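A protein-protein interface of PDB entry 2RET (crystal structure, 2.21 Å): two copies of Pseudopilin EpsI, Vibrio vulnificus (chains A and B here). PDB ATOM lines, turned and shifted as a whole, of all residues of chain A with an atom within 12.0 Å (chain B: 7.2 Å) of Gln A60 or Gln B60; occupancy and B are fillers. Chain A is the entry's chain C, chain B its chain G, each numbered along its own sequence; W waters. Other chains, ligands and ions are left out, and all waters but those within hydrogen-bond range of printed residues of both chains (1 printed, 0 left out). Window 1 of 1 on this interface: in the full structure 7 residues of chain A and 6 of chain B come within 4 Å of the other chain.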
ATOM      1  N   MET A  29      -8.600 -39.930 -22.667  1.00  0.00           N
ATOM      2  CA  MET A  29      -9.967 -40.067 -22.167  1.00  0.00           C
ATOM      3  C   MET A  29     -10.213 -41.383 -21.484  1.00  0.00           C
ATOM      4  O   MET A  29     -11.011 -41.433 -20.563  1.00  0.00           O
ATOM      5  CB  MET A  29     -10.983 -39.910 -23.304  1.00  0.00           C
ATOM      6  CG  MET A  29     -11.138 -38.503 -23.840  1.00  0.00           C
ATOM      7  SD  MET A  29     -11.658 -37.212 -22.460  1.00  0.00           S
ATOM      8  CE  MET A  29     -11.896 -35.713 -23.657  1.00  0.00           C
ATOM      9  N   PRO A  55      -1.901 -30.758 -19.916  1.00  0.00           N
ATOM     10  CA  PRO A  55      -2.978 -30.175 -19.097  1.00  0.00           C
ATOM     11  C   PRO A  55      -3.108 -28.668 -19.254  1.00  0.00           C
ATOM     12  O   PRO A  55      -2.123 -27.959 -19.491  1.00  0.00           O
ATOM     13  CB  PRO A  55      -2.576 -30.521 -17.664  1.00  0.00           C
ATOM     14  CG  PRO A  55      -1.736 -31.760 -17.811  1.00  0.00           C
ATOM     15  CD  PRO A  55      -0.992 -31.591 -19.113  1.00  0.00           C
ATOM     16  N   VAL A  56      -4.338 -28.204 -19.162  1.00  0.00           N
ATOM     17  CA  VAL A  56      -4.647 -26.808 -19.322  1.00  0.00           C
ATOM     18  C   VAL A  56      -5.424 -26.370 -18.075  1.00  0.00           C
ATOM     19  O   VAL A  56      -6.406 -27.016 -17.679  1.00  0.00           O
ATOM     20  CB  VAL A  56      -5.477 -26.565 -20.592  1.00  0.00           C
ATOM     21  CG1 VAL A  56      -5.769 -25.087 -20.760  1.00  0.00           C
ATOM     22  CG2 VAL A  56      -4.778 -27.127 -21.804  1.00  0.00           C
ATOM     23  N   ALA A  57      -4.969 -25.277 -17.459  1.00  0.00           N
ATOM     24  CA  ALA A  57      -5.577 -24.760 -16.244  1.00  0.00           C
ATOM     25  C   ALA A  57      -7.000 -24.301 -16.522  1.00  0.00           C
ATOM     26  O   ALA A  57      -7.315 -23.851 -17.626  1.00  0.00           O
ATOM     27  CB  ALA A  57      -4.752 -23.621 -15.692  1.00  0.00           C
ATOM     28  N   THR A  58      -7.860 -24.433 -15.513  1.00  0.00           N
ATOM     29  CA  THR A  58      -9.254 -23.996 -15.609  1.00  0.00           C
ATOM     30  C   THR A  58      -9.737 -23.345 -14.302  1.00  0.00           C
ATOM     31  O   THR A  58     -10.051 -24.023 -13.322  1.00  0.00           O
ATOM     32  CB  THR A  58     -10.205 -25.149 -16.063  1.00  0.00           C
ATOM     33  OG1 THR A  58     -11.379 -25.176 -15.237  1.00  0.00           O
ATOM     34  CG2 THR A  58      -9.509 -26.500 -16.015  1.00  0.00           C
ATOM     35  N   GLN A  60     -12.251 -22.875 -12.880  1.00  0.00           N
ATOM     36  CA  GLN A  60     -13.342 -23.612 -12.259  1.00  0.00           C
ATOM     37  C   GLN A  60     -12.930 -25.015 -11.766  1.00  0.00           C
ATOM     38  O   GLN A  60     -11.946 -25.596 -12.259  1.00  0.00           O
ATOM     39  CB  GLN A  60     -14.500 -23.748 -13.247  1.00  0.00           C
ATOM     40  CG  GLN A  60     -14.397 -24.941 -14.204  1.00  0.00           C
ATOM     41  CD  GLN A  60     -15.730 -25.350 -14.809  1.00  0.00           C
ATOM     42  OE1 GLN A  60     -15.814 -25.621 -16.002  1.00  0.00           O
ATOM     43  NE2 GLN A  60     -16.766 -25.411 -13.995  1.00  0.00           N
ATOM     44  N   PRO A  61     -13.714 -25.587 -10.821  1.00  0.00           N
ATOM     45  CA  PRO A  61     -13.405 -26.904 -10.246  1.00  0.00           C
ATOM     46  C   PRO A  61     -14.022 -28.103 -10.987  1.00  0.00           C
ATOM     47  O   PRO A  61     -13.723 -29.253 -10.663  1.00  0.00           O
ATOM     48  CB  PRO A  61     -14.001 -26.794  -8.841  1.00  0.00           C
ATOM     49  CG  PRO A  61     -15.193 -25.924  -9.024  1.00  0.00           C
ATOM     50  CD  PRO A  61     -14.945 -25.031 -10.224  1.00  0.00           C
ATOM     51  N   LEU A  62     -14.849 -27.841 -11.992  1.00  0.00           N
ATOM     52  CA  LEU A  62     -15.715 -28.884 -12.564  1.00  0.00           C
ATOM     53  C   LEU A  62     -15.042 -29.649 -13.735  1.00  0.00           C
ATOM     54  O   LEU A  62     -15.159 -30.877 -13.878  1.00  0.00           O
ATOM     55  CB  LEU A  62     -17.066 -28.247 -12.986  1.00  0.00           C
ATOM     56  CG  LEU A  62     -17.704 -27.273 -11.997  1.00  0.00           C
ATOM     57  CD1 LEU A  62     -18.916 -26.559 -12.550  1.00  0.00           C
ATOM     58  CD2 LEU A  62     -18.083 -28.003 -10.711  1.00  0.00           C
ATOM     59  N   LEU A  63     -14.307 -28.931 -14.559  1.00  0.00           N
ATOM     60  CA  LEU A  63     -13.730 -29.523 -15.748  1.00  0.00           C
ATOM     61  C   LEU A  63     -12.197 -29.558 -15.692  1.00  0.00           C
ATOM     62  O   LEU A  63     -11.568 -28.639 -15.161  1.00  0.00           O
ATOM     63  CB  LEU A  63     -14.195 -28.726 -16.964  1.00  0.00           C
ATOM     64  CG  LEU A  63     -15.712 -28.659 -17.134  1.00  0.00           C
ATOM     65  CD1 LEU A  63     -16.061 -27.766 -18.282  1.00  0.00           C
ATOM     66  CD2 LEU A  63     -16.299 -30.050 -17.338  1.00  0.00           C
ATOM     67  N   LYS A  64     -11.607 -30.637 -16.203  1.00  0.00           N
ATOM     68  CA  LYS A  64     -10.183 -30.640 -16.551  1.00  0.00           C
ATOM     69  C   LYS A  64     -10.067 -30.444 -18.067  1.00  0.00           C
ATOM     70  O   LYS A  64     -10.967 -30.810 -18.799  1.00  0.00           O
ATOM     71  CB  LYS A  64      -9.495 -31.946 -16.126  1.00  0.00           C
ATOM     72  CG  LYS A  64      -9.470 -32.173 -14.610  1.00  0.00           C
ATOM     73  CD  LYS A  64      -8.315 -33.130 -14.189  1.00  0.00           C
ATOM     74  CE  LYS A  64      -8.773 -34.560 -13.831  1.00  0.00           C
ATOM     75  NZ  LYS A  64      -8.963 -34.734 -12.325  1.00  0.00           N
ATOM     76  N   ALA A  65      -8.988 -29.824 -18.517  1.00  0.00           N
ATOM     77  CA  ALA A  65      -8.740 -29.601 -19.927  1.00  0.00           C
ATOM     78  C   ALA A  65      -7.364 -30.167 -20.287  1.00  0.00           C
ATOM     79  O   ALA A  65      -6.463 -30.196 -19.467  1.00  0.00           O
ATOM     80  CB  ALA A  65      -8.821 -28.111 -20.272  1.00  0.00           C
ATOM     81  N   PHE A  66      -7.233 -30.666 -21.509  1.00  0.00           N
ATOM     82  CA  PHE A  66      -5.923 -31.052 -22.022  1.00  0.00           C
ATOM     83  C   PHE A  66      -5.898 -30.673 -23.484  1.00  0.00           C
ATOM     84  O   PHE A  66      -6.934 -30.677 -24.155  1.00  0.00           O
ATOM     85  CB  PHE A  66      -5.611 -32.558 -21.806  1.00  0.00           C
ATOM     86  CG  PHE A  66      -6.510 -33.496 -22.588  1.00  0.00           C
ATOM     87  CD1 PHE A  66      -7.720 -33.914 -22.059  1.00  0.00           C
ATOM     88  CD2 PHE A  66      -6.152 -33.954 -23.851  1.00  0.00           C
ATOM     89  CE1 PHE A  66      -8.564 -34.759 -22.805  1.00  0.00           C
ATOM     90  CE2 PHE A  66      -7.029 -34.810 -24.636  1.00  0.00           C
ATOM     91  CZ  PHE A  66      -8.182 -35.204 -24.115  1.00  0.00           C
ATOM     92  N   ASP A  67      -4.703 -30.325 -23.943  1.00  0.00           N
ATOM     93  CA  ASP A  67      -4.414 -30.115 -25.362  1.00  0.00           C
ATOM     94  C   ASP A  67      -3.623 -31.289 -25.881  1.00  0.00           C
ATOM     95  O   ASP A  67      -2.685 -31.740 -25.242  1.00  0.00           O
ATOM     96  CB  ASP A  67      -3.553 -28.878 -25.528  1.00  0.00           C
ATOM     97  CG  ASP A  67      -4.337 -27.605 -25.437  1.00  0.00           C
ATOM     98  OD1 ASP A  67      -5.542 -27.620 -25.758  1.00  0.00           O
ATOM     99  OD2 ASP A  67      -3.736 -26.574 -25.077  1.00  0.00           O
ATOM    100  N   VAL A  82      -5.608 -29.877 -30.573  1.00  0.00           N
ATOM    101  CA  VAL A  82      -6.988 -30.057 -30.172  1.00  0.00           C
ATOM    102  C   VAL A  82      -7.080 -30.020 -28.644  1.00  0.00           C
ATOM    103  O   VAL A  82      -6.284 -30.645 -27.959  1.00  0.00           O
ATOM    104  CB  VAL A  82      -7.562 -31.404 -30.629  1.00  0.00           C
ATOM    105  CG1 VAL A  82      -9.023 -31.444 -30.243  1.00  0.00           C
ATOM    106  CG2 VAL A  82      -7.439 -31.574 -32.122  1.00  0.00           C
ATOM    107  N   ARG A  83      -8.053 -29.268 -28.145  1.00  0.00           N
ATOM    108  CA  ARG A  83      -8.359 -29.181 -26.737  1.00  0.00           C
ATOM    109  C   ARG A  83      -9.632 -29.952 -26.414  1.00  0.00           C
ATOM    110  O   ARG A  83     -10.584 -29.893 -27.156  1.00  0.00           O
ATOM    111  CB  ARG A  83      -8.560 -27.718 -26.344  1.00  0.00           C
ATOM    112  CG  ARG A  83      -8.935 -27.524 -24.872  1.00  0.00           C
ATOM    113  CD  ARG A  83      -8.782 -26.086 -24.477  1.00  0.00           C
ATOM    114  NE  ARG A  83      -7.390 -25.671 -24.538  1.00  0.00           N
ATOM    115  CZ  ARG A  83      -6.917 -24.522 -24.062  1.00  0.00           C
ATOM    116  NH1 ARG A  83      -7.717 -23.650 -23.453  1.00  0.00           N
ATOM    117  NH2 ARG A  83      -5.621 -24.259 -24.166  1.00  0.00           N
ATOM    118  N   SER A  84      -9.622 -30.685 -25.306  1.00  0.00           N
ATOM    119  CA  SER A  84     -10.767 -31.436 -24.845  1.00  0.00           C
ATOM    120  C   SER A  84     -10.917 -31.259 -23.366  1.00  0.00           C
ATOM    121  O   SER A  84      -9.966 -30.908 -22.698  1.00  0.00           O
ATOM    122  CB  SER A  84     -10.609 -32.921 -25.133  1.00  0.00           C
ATOM    123  OG  SER A  84     -10.678 -33.163 -26.526  1.00  0.00           O
ATOM    124  N   TYR A  85     -12.144 -31.483 -22.883  1.00  0.00           N
ATOM    125  CA  TYR A  85     -12.492 -31.317 -21.477  1.00  0.00           C
ATOM    126  C   TYR A  85     -13.060 -32.582 -20.890  1.00  0.00           C
ATOM    127  O   TYR A  85     -13.816 -33.319 -21.541  1.00  0.00           O
ATOM    128  CB  TYR A  85     -13.491 -30.198 -21.269  1.00  0.00           C
ATOM    129  CG  TYR A  85     -13.015 -28.882 -21.773  1.00  0.00           C
ATOM    130  CD1 TYR A  85     -12.506 -27.927 -20.900  1.00  0.00           C
ATOM    131  CD2 TYR A  85     -13.058 -28.590 -23.126  1.00  0.00           C
ATOM    132  CE1 TYR A  85     -12.071 -26.718 -21.355  1.00  0.00           C
ATOM    133  CE2 TYR A  85     -12.620 -27.383 -23.595  1.00  0.00           C
ATOM    134  CZ  TYR A  85     -12.126 -26.456 -22.707  1.00  0.00           C
ATOM    135  OH  TYR A  85     -11.703 -25.248 -23.165  1.00  0.00           O
ATOM    136  N   VAL A  86     -12.696 -32.800 -19.630  1.00  0.00           N
ATOM    137  CA  VAL A  86     -13.046 -34.000 -18.888  1.00  0.00           C
ATOM    138  C   VAL A  86     -13.679 -33.593 -17.564  1.00  0.00           C
ATOM    139  O   VAL A  86     -13.284 -32.595 -16.953  1.00  0.00           O
ATOM    140  CB  VAL A  86     -11.786 -34.872 -18.650  1.00  0.00           C
ATOM    141  CG1 VAL A  86     -12.169 -36.290 -18.309  1.00  0.00           C
ATOM    142  CG2 VAL A  86     -10.955 -34.876 -19.863  1.00  0.00           C
ATOM    143  N   ALA A  87     -14.699 -34.331 -17.148  1.00  0.00           N
ATOM    144  CA  ALA A  87     -15.393 -34.044 -15.903  1.00  0.00           C
ATOM    145  C   ALA A  87     -14.497 -34.402 -14.706  1.00  0.00           C
ATOM    146  O   ALA A  87     -13.897 -35.475 -14.702  1.00  0.00           O
ATOM    147  CB  ALA A  87     -16.700 -34.836 -15.852  1.00  0.00           C
ATOM    148  N   SER A  88     -14.374 -33.506 -13.716  1.00  0.00           N
ATOM    149  CA  SER A  88     -13.719 -33.867 -12.430  1.00  0.00           C
ATOM    150  C   SER A  88     -14.688 -34.612 -11.508  1.00  0.00           C
ATOM    151  O   SER A  88     -14.300 -35.579 -10.841  1.00  0.00           O
ATOM    152  CB  SER A  88     -13.170 -32.639 -11.699  1.00  0.00           C
ATOM    153  OG  SER A  88     -12.063 -32.092 -12.388  1.00  0.00           O
ATOM    154  N   ALA B  57     -14.642 -14.561 -15.527  1.00  0.00           N
ATOM    155  CA  ALA B  57     -13.921 -15.085 -16.681  1.00  0.00           C
ATOM    156  C   ALA B  57     -13.751 -16.595 -16.556  1.00  0.00           C
ATOM    157  O   ALA B  57     -13.551 -17.119 -15.457  1.00  0.00           O
ATOM    158  CB  ALA B  57     -12.569 -14.415 -16.799  1.00  0.00           C
ATOM    159  N   THR B  58     -13.809 -17.289 -17.694  1.00  0.00           N
ATOM    160  CA  THR B  58     -13.696 -18.747 -17.716  1.00  0.00           C
ATOM    161  C   THR B  58     -12.698 -19.231 -18.777  1.00  0.00           C
ATOM    162  O   THR B  58     -12.570 -18.646 -19.862  1.00  0.00           O
ATOM    163  CB  THR B  58     -15.102 -19.442 -17.831  1.00  0.00           C
ATOM    164  OG1 THR B  58     -15.112 -20.404 -18.896  1.00  0.00           O
ATOM    165  CG2 THR B  58     -16.207 -18.418 -18.054  1.00  0.00           C
ATOM    166  N   THR B  59     -11.988 -20.310 -18.451  1.00  0.00           N
ATOM    167  CA  THR B  59     -10.853 -20.779 -19.261  1.00  0.00           C
ATOM    168  C   THR B  59     -11.311 -21.631 -20.440  1.00  0.00           C
ATOM    169  O   THR B  59     -10.597 -22.539 -20.889  1.00  0.00           O
ATOM    170  CB  THR B  59      -9.854 -21.597 -18.409  1.00  0.00           C
ATOM    171  OG1 THR B  59      -9.806 -21.077 -17.071  1.00  0.00           O
ATOM    172  CG2 THR B  59      -8.448 -21.564 -19.049  1.00  0.00           C
ATOM    173  N   GLN B  60     -12.496 -21.317 -20.947  1.00  0.00           N
ATOM    174  CA  GLN B  60     -13.135 -22.108 -21.971  1.00  0.00           C
ATOM    175  C   GLN B  60     -14.307 -21.340 -22.598  1.00  0.00           C
ATOM    176  O   GLN B  60     -14.782 -20.344 -22.029  1.00  0.00           O
ATOM    177  CB  GLN B  60     -13.632 -23.421 -21.366  1.00  0.00           C
ATOM    178  CG  GLN B  60     -14.842 -23.279 -20.455  1.00  0.00           C
ATOM    179  CD  GLN B  60     -15.387 -24.621 -20.016  1.00  0.00           C
ATOM    180  OE1 GLN B  60     -15.681 -24.819 -18.840  1.00  0.00           O
ATOM    181  NE2 GLN B  60     -15.508 -25.556 -20.951  1.00  0.00           N
ATOM    182  N   PRO B  61     -14.786 -21.809 -23.765  1.00  0.00           N
ATOM    183  CA  PRO B  61     -15.918 -21.182 -24.437  1.00  0.00           C
ATOM    184  C   PRO B  61     -17.281 -21.733 -24.004  1.00  0.00           C
ATOM    185  O   PRO B  61     -18.310 -21.105 -24.231  1.00  0.00           O
ATOM    186  CB  PRO B  61     -15.646 -21.497 -25.915  1.00  0.00           C
ATOM    187  CG  PRO B  61     -14.915 -22.786 -25.892  1.00  0.00           C
ATOM    188  CD  PRO B  61     -14.270 -22.953 -24.538  1.00  0.00           C
ATOM    189  N   LEU B  62     -17.272 -22.875 -23.338  1.00  0.00           N
ATOM    190  CA  LEU B  62     -18.494 -23.663 -23.111  1.00  0.00           C
ATOM    191  C   LEU B  62     -19.370 -23.085 -21.953  1.00  0.00           C
ATOM    192  O   LEU B  62     -20.618 -22.956 -22.036  1.00  0.00           O
ATOM    193  CB  LEU B  62     -18.093 -25.141 -22.835  1.00  0.00           C
ATOM    194  CG  LEU B  62     -16.888 -25.757 -23.582  1.00  0.00           C
ATOM    195  CD1 LEU B  62     -16.601 -27.169 -23.138  1.00  0.00           C
ATOM    196  CD2 LEU B  62     -17.080 -25.706 -25.094  1.00  0.00           C
ATOM    197  N   LEU B  63     -18.711 -22.718 -20.868  1.00  0.00           N
ATOM    198  CA  LEU B  63     -19.431 -22.264 -19.702  1.00  0.00           C
ATOM    199  C   LEU B  63     -19.221 -20.782 -19.449  1.00  0.00           C
ATOM    200  O   LEU B  63     -18.138 -20.258 -19.680  1.00  0.00           O
ATOM    201  CB  LEU B  63     -18.982 -23.074 -18.490  1.00  0.00           C
ATOM    202  CG  LEU B  63     -19.100 -24.601 -18.554  1.00  0.00           C
ATOM    203  CD1 LEU B  63     -18.823 -25.122 -17.191  1.00  0.00           C
ATOM    204  CD2 LEU B  63     -20.455 -25.098 -19.040  1.00  0.00           C
ATOM    205  N   LYS B  64     -20.263 -20.114 -18.954  1.00  0.00           N
ATOM    206  CA  LYS B  64     -20.125 -18.796 -18.340  1.00  0.00           C
ATOM    207  C   LYS B  64     -20.279 -18.951 -16.813  1.00  0.00           C
ATOM    208  O   LYS B  64     -20.992 -19.836 -16.365  1.00  0.00           O
ATOM    209  CB  LYS B  64     -21.176 -17.828 -18.899  1.00  0.00           C
ATOM    210  CG  LYS B  64     -21.181 -17.763 -20.420  1.00  0.00           C
ATOM    211  CD  LYS B  64     -21.698 -16.406 -20.958  1.00  0.00           C
ATOM    212  CE  LYS B  64     -23.191 -16.428 -21.371  1.00  0.00           C
ATOM    213  NZ  LYS B  64     -23.432 -15.610 -22.620  1.00  0.00           N
ATOM    214  N   ALA B  65     -19.574 -18.129 -16.041  1.00  0.00           N
ATOM    215  CA  ALA B  65     -19.726 -18.100 -14.597  1.00  0.00           C
ATOM    216  C   ALA B  65     -20.222 -16.738 -14.106  1.00  0.00           C
ATOM    217  O   ALA B  65     -20.047 -15.726 -14.739  1.00  0.00           O
ATOM    218  CB  ALA B  65     -18.414 -18.459 -13.901  1.00  0.00           C
ATOM    219  N   ARG B  83     -20.962 -18.935  -6.461  1.00  0.00           N
ATOM    220  CA  ARG B  83     -20.570 -19.021  -7.868  1.00  0.00           C
ATOM    221  C   ARG B  83     -21.389 -20.078  -8.553  1.00  0.00           C
ATOM    222  O   ARG B  83     -21.584 -21.162  -8.000  1.00  0.00           O
ATOM    223  CB  ARG B  83     -19.097 -19.413  -8.019  1.00  0.00           C
ATOM    224  CG  ARG B  83     -18.611 -19.380  -9.440  1.00  0.00           C
ATOM    225  CD  ARG B  83     -17.114 -19.343  -9.464  1.00  0.00           C
ATOM    226  NE  ARG B  83     -16.572 -18.010  -9.236  1.00  0.00           N
ATOM    227  CZ  ARG B  83     -15.279 -17.739  -9.064  1.00  0.00           C
ATOM    228  NH1 ARG B  83     -14.369 -18.708  -9.093  1.00  0.00           N
ATOM    229  NH2 ARG B  83     -14.885 -16.490  -8.867  1.00  0.00           N
ATOM    230  N   TYR B  85     -22.460 -21.618 -12.766  1.00  0.00           N
ATOM    231  CA  TYR B  85     -22.085 -21.748 -14.183  1.00  0.00           C
ATOM    232  C   TYR B  85     -23.313 -22.023 -15.010  1.00  0.00           C
ATOM    233  O   TYR B  85     -24.217 -22.754 -14.582  1.00  0.00           O
ATOM    234  CB  TYR B  85     -21.060 -22.872 -14.414  1.00  0.00           C
ATOM    235  CG  TYR B  85     -19.856 -22.699 -13.538  1.00  0.00           C
ATOM    236  CD1 TYR B  85     -18.683 -22.149 -14.028  1.00  0.00           C
ATOM    237  CD2 TYR B  85     -19.920 -23.028 -12.188  1.00  0.00           C
ATOM    238  CE1 TYR B  85     -17.596 -21.948 -13.196  1.00  0.00           C
ATOM    239  CE2 TYR B  85     -18.857 -22.828 -11.355  1.00  0.00           C
ATOM    240  CZ  TYR B  85     -17.697 -22.295 -11.859  1.00  0.00           C
ATOM    241  OH  TYR B  85     -16.640 -22.126 -10.999  1.00  0.00           O
HETATM  242  O   HOH W   1     -13.855 -23.598 -17.131  1.00  0.00           O
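Water W1 lies within hydrogen-bond range of the side-chain amide oxygen of Gln B60, the side-chain amide oxygen of Gln A60 and the side-chain hydroxyl of Thr A58.
The side-chain amide oxygen (OE1) of Gln A60 sits close to the side-chain amide oxygen (OE1) of Gln B60.
Among the printed residues, pairs that only touch across the chains: Ala A57 with Thr B59, Leu A63 with Gln B60, Tyr A85 with Gln B60, Gln A60 with Leu B63, Thr A58 with Thr B59, Pro A61 with Tyr B85, Gln A60 with Tyr B85, Leu A62 with Tyr B85, Tyr A85 with Pro B61, Tyr A85 with Thr B59, Tyr A85 with Leu B62 and Leu A63 with Leu B63.
Along chain B the printed residues that touch a printed residue of chain A span positions 59 to 85.
Among the printed residues, 13 pairs touch across the chains.
Among the printed residues, no Asp or Glu carboxylate lies within 4 Å of a Lys or Arg side-chain nitrogen of the other chain.
Of chain B, only Gln B60, Leu B63 and Tyr B85 come within 4 Å of Gln A60.
Of chain A, only Gln A60 (3.0 Å), Leu A63 (3.0 Å) and Tyr A85 (3.2 Å) come within 4 Å of Gln B60.
No residue of chain A comes within 4 Å of Thr B58.
Of the printed residues of chain A, Pro B61 touches Tyr A85.
Of the printed residues of chain A, Tyr B85 touches Gln A60 (3.5 Å), Pro A61 (3.5 Å) and Leu A62 (3.7 Å).
Printed residues of chain B within 4 Å of Thr A58: Thr B59.
Printed residues of chain B within 4 Å of Ala A57: Thr B59 (2.9 Å).
Printed residues of chain B within 4 Å of Pro A61: Tyr B85 (3.5 Å).
Printed residues of chain B within 4 Å of Leu A62: Tyr B85 (3.7 Å).
Printed residues of chain B within 4 Å of Leu A63: Gln B60 and Leu B63.
Phe A66 touches none of the printed residues of chain B.
The nearest residue of chain B that does not touch Gln A60 is Thr B59 (5.2 Å).
The nearest printed residue of chain B that does not touch Ala A57 is Gln B60 (6.7 Å).
Gln B60 touches its own counterpart, Gln A60.
Gln A60 touches Leu B63, and with the chains exchanged Leu A63 touches Gln B60.
Leu A62 touches Tyr B85, and with the chains exchanged Tyr A85 touches Leu B62.
Leu B63 touches its own counterpart, Leu A63.
Positions printed for both chains: 57, 58, 60, 61, 62, 63, 64, 65, 83 and 85.
Of the 13 pairs that touch across the chains among the printed residues, 10 have their exchanged pair printed and touching as well.
The side-chain hydroxyl of Thr A58 lies within hydrogen-bond range of the backbone carbonyl oxygen of Gln A60, at 3.1 Å.
The backbone carbonyl oxygen (O) of Leu A63 lies close to the side-chain hydroxyl (OG1) of Thr A58, 3.5 Å away.
N of Ser A88 lies within hydrogen-bond range of O of Leu A62, at 2.7 Å.
The side-chain hydroxyl of Thr B58 sits at hydrogen-bond distance from the backbone carbonyl oxygen of Gln B60.
The side-chain hydroxyl (OG1) of Thr B58 lies close to the backbone carbonyl oxygen (O) of Leu B63.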
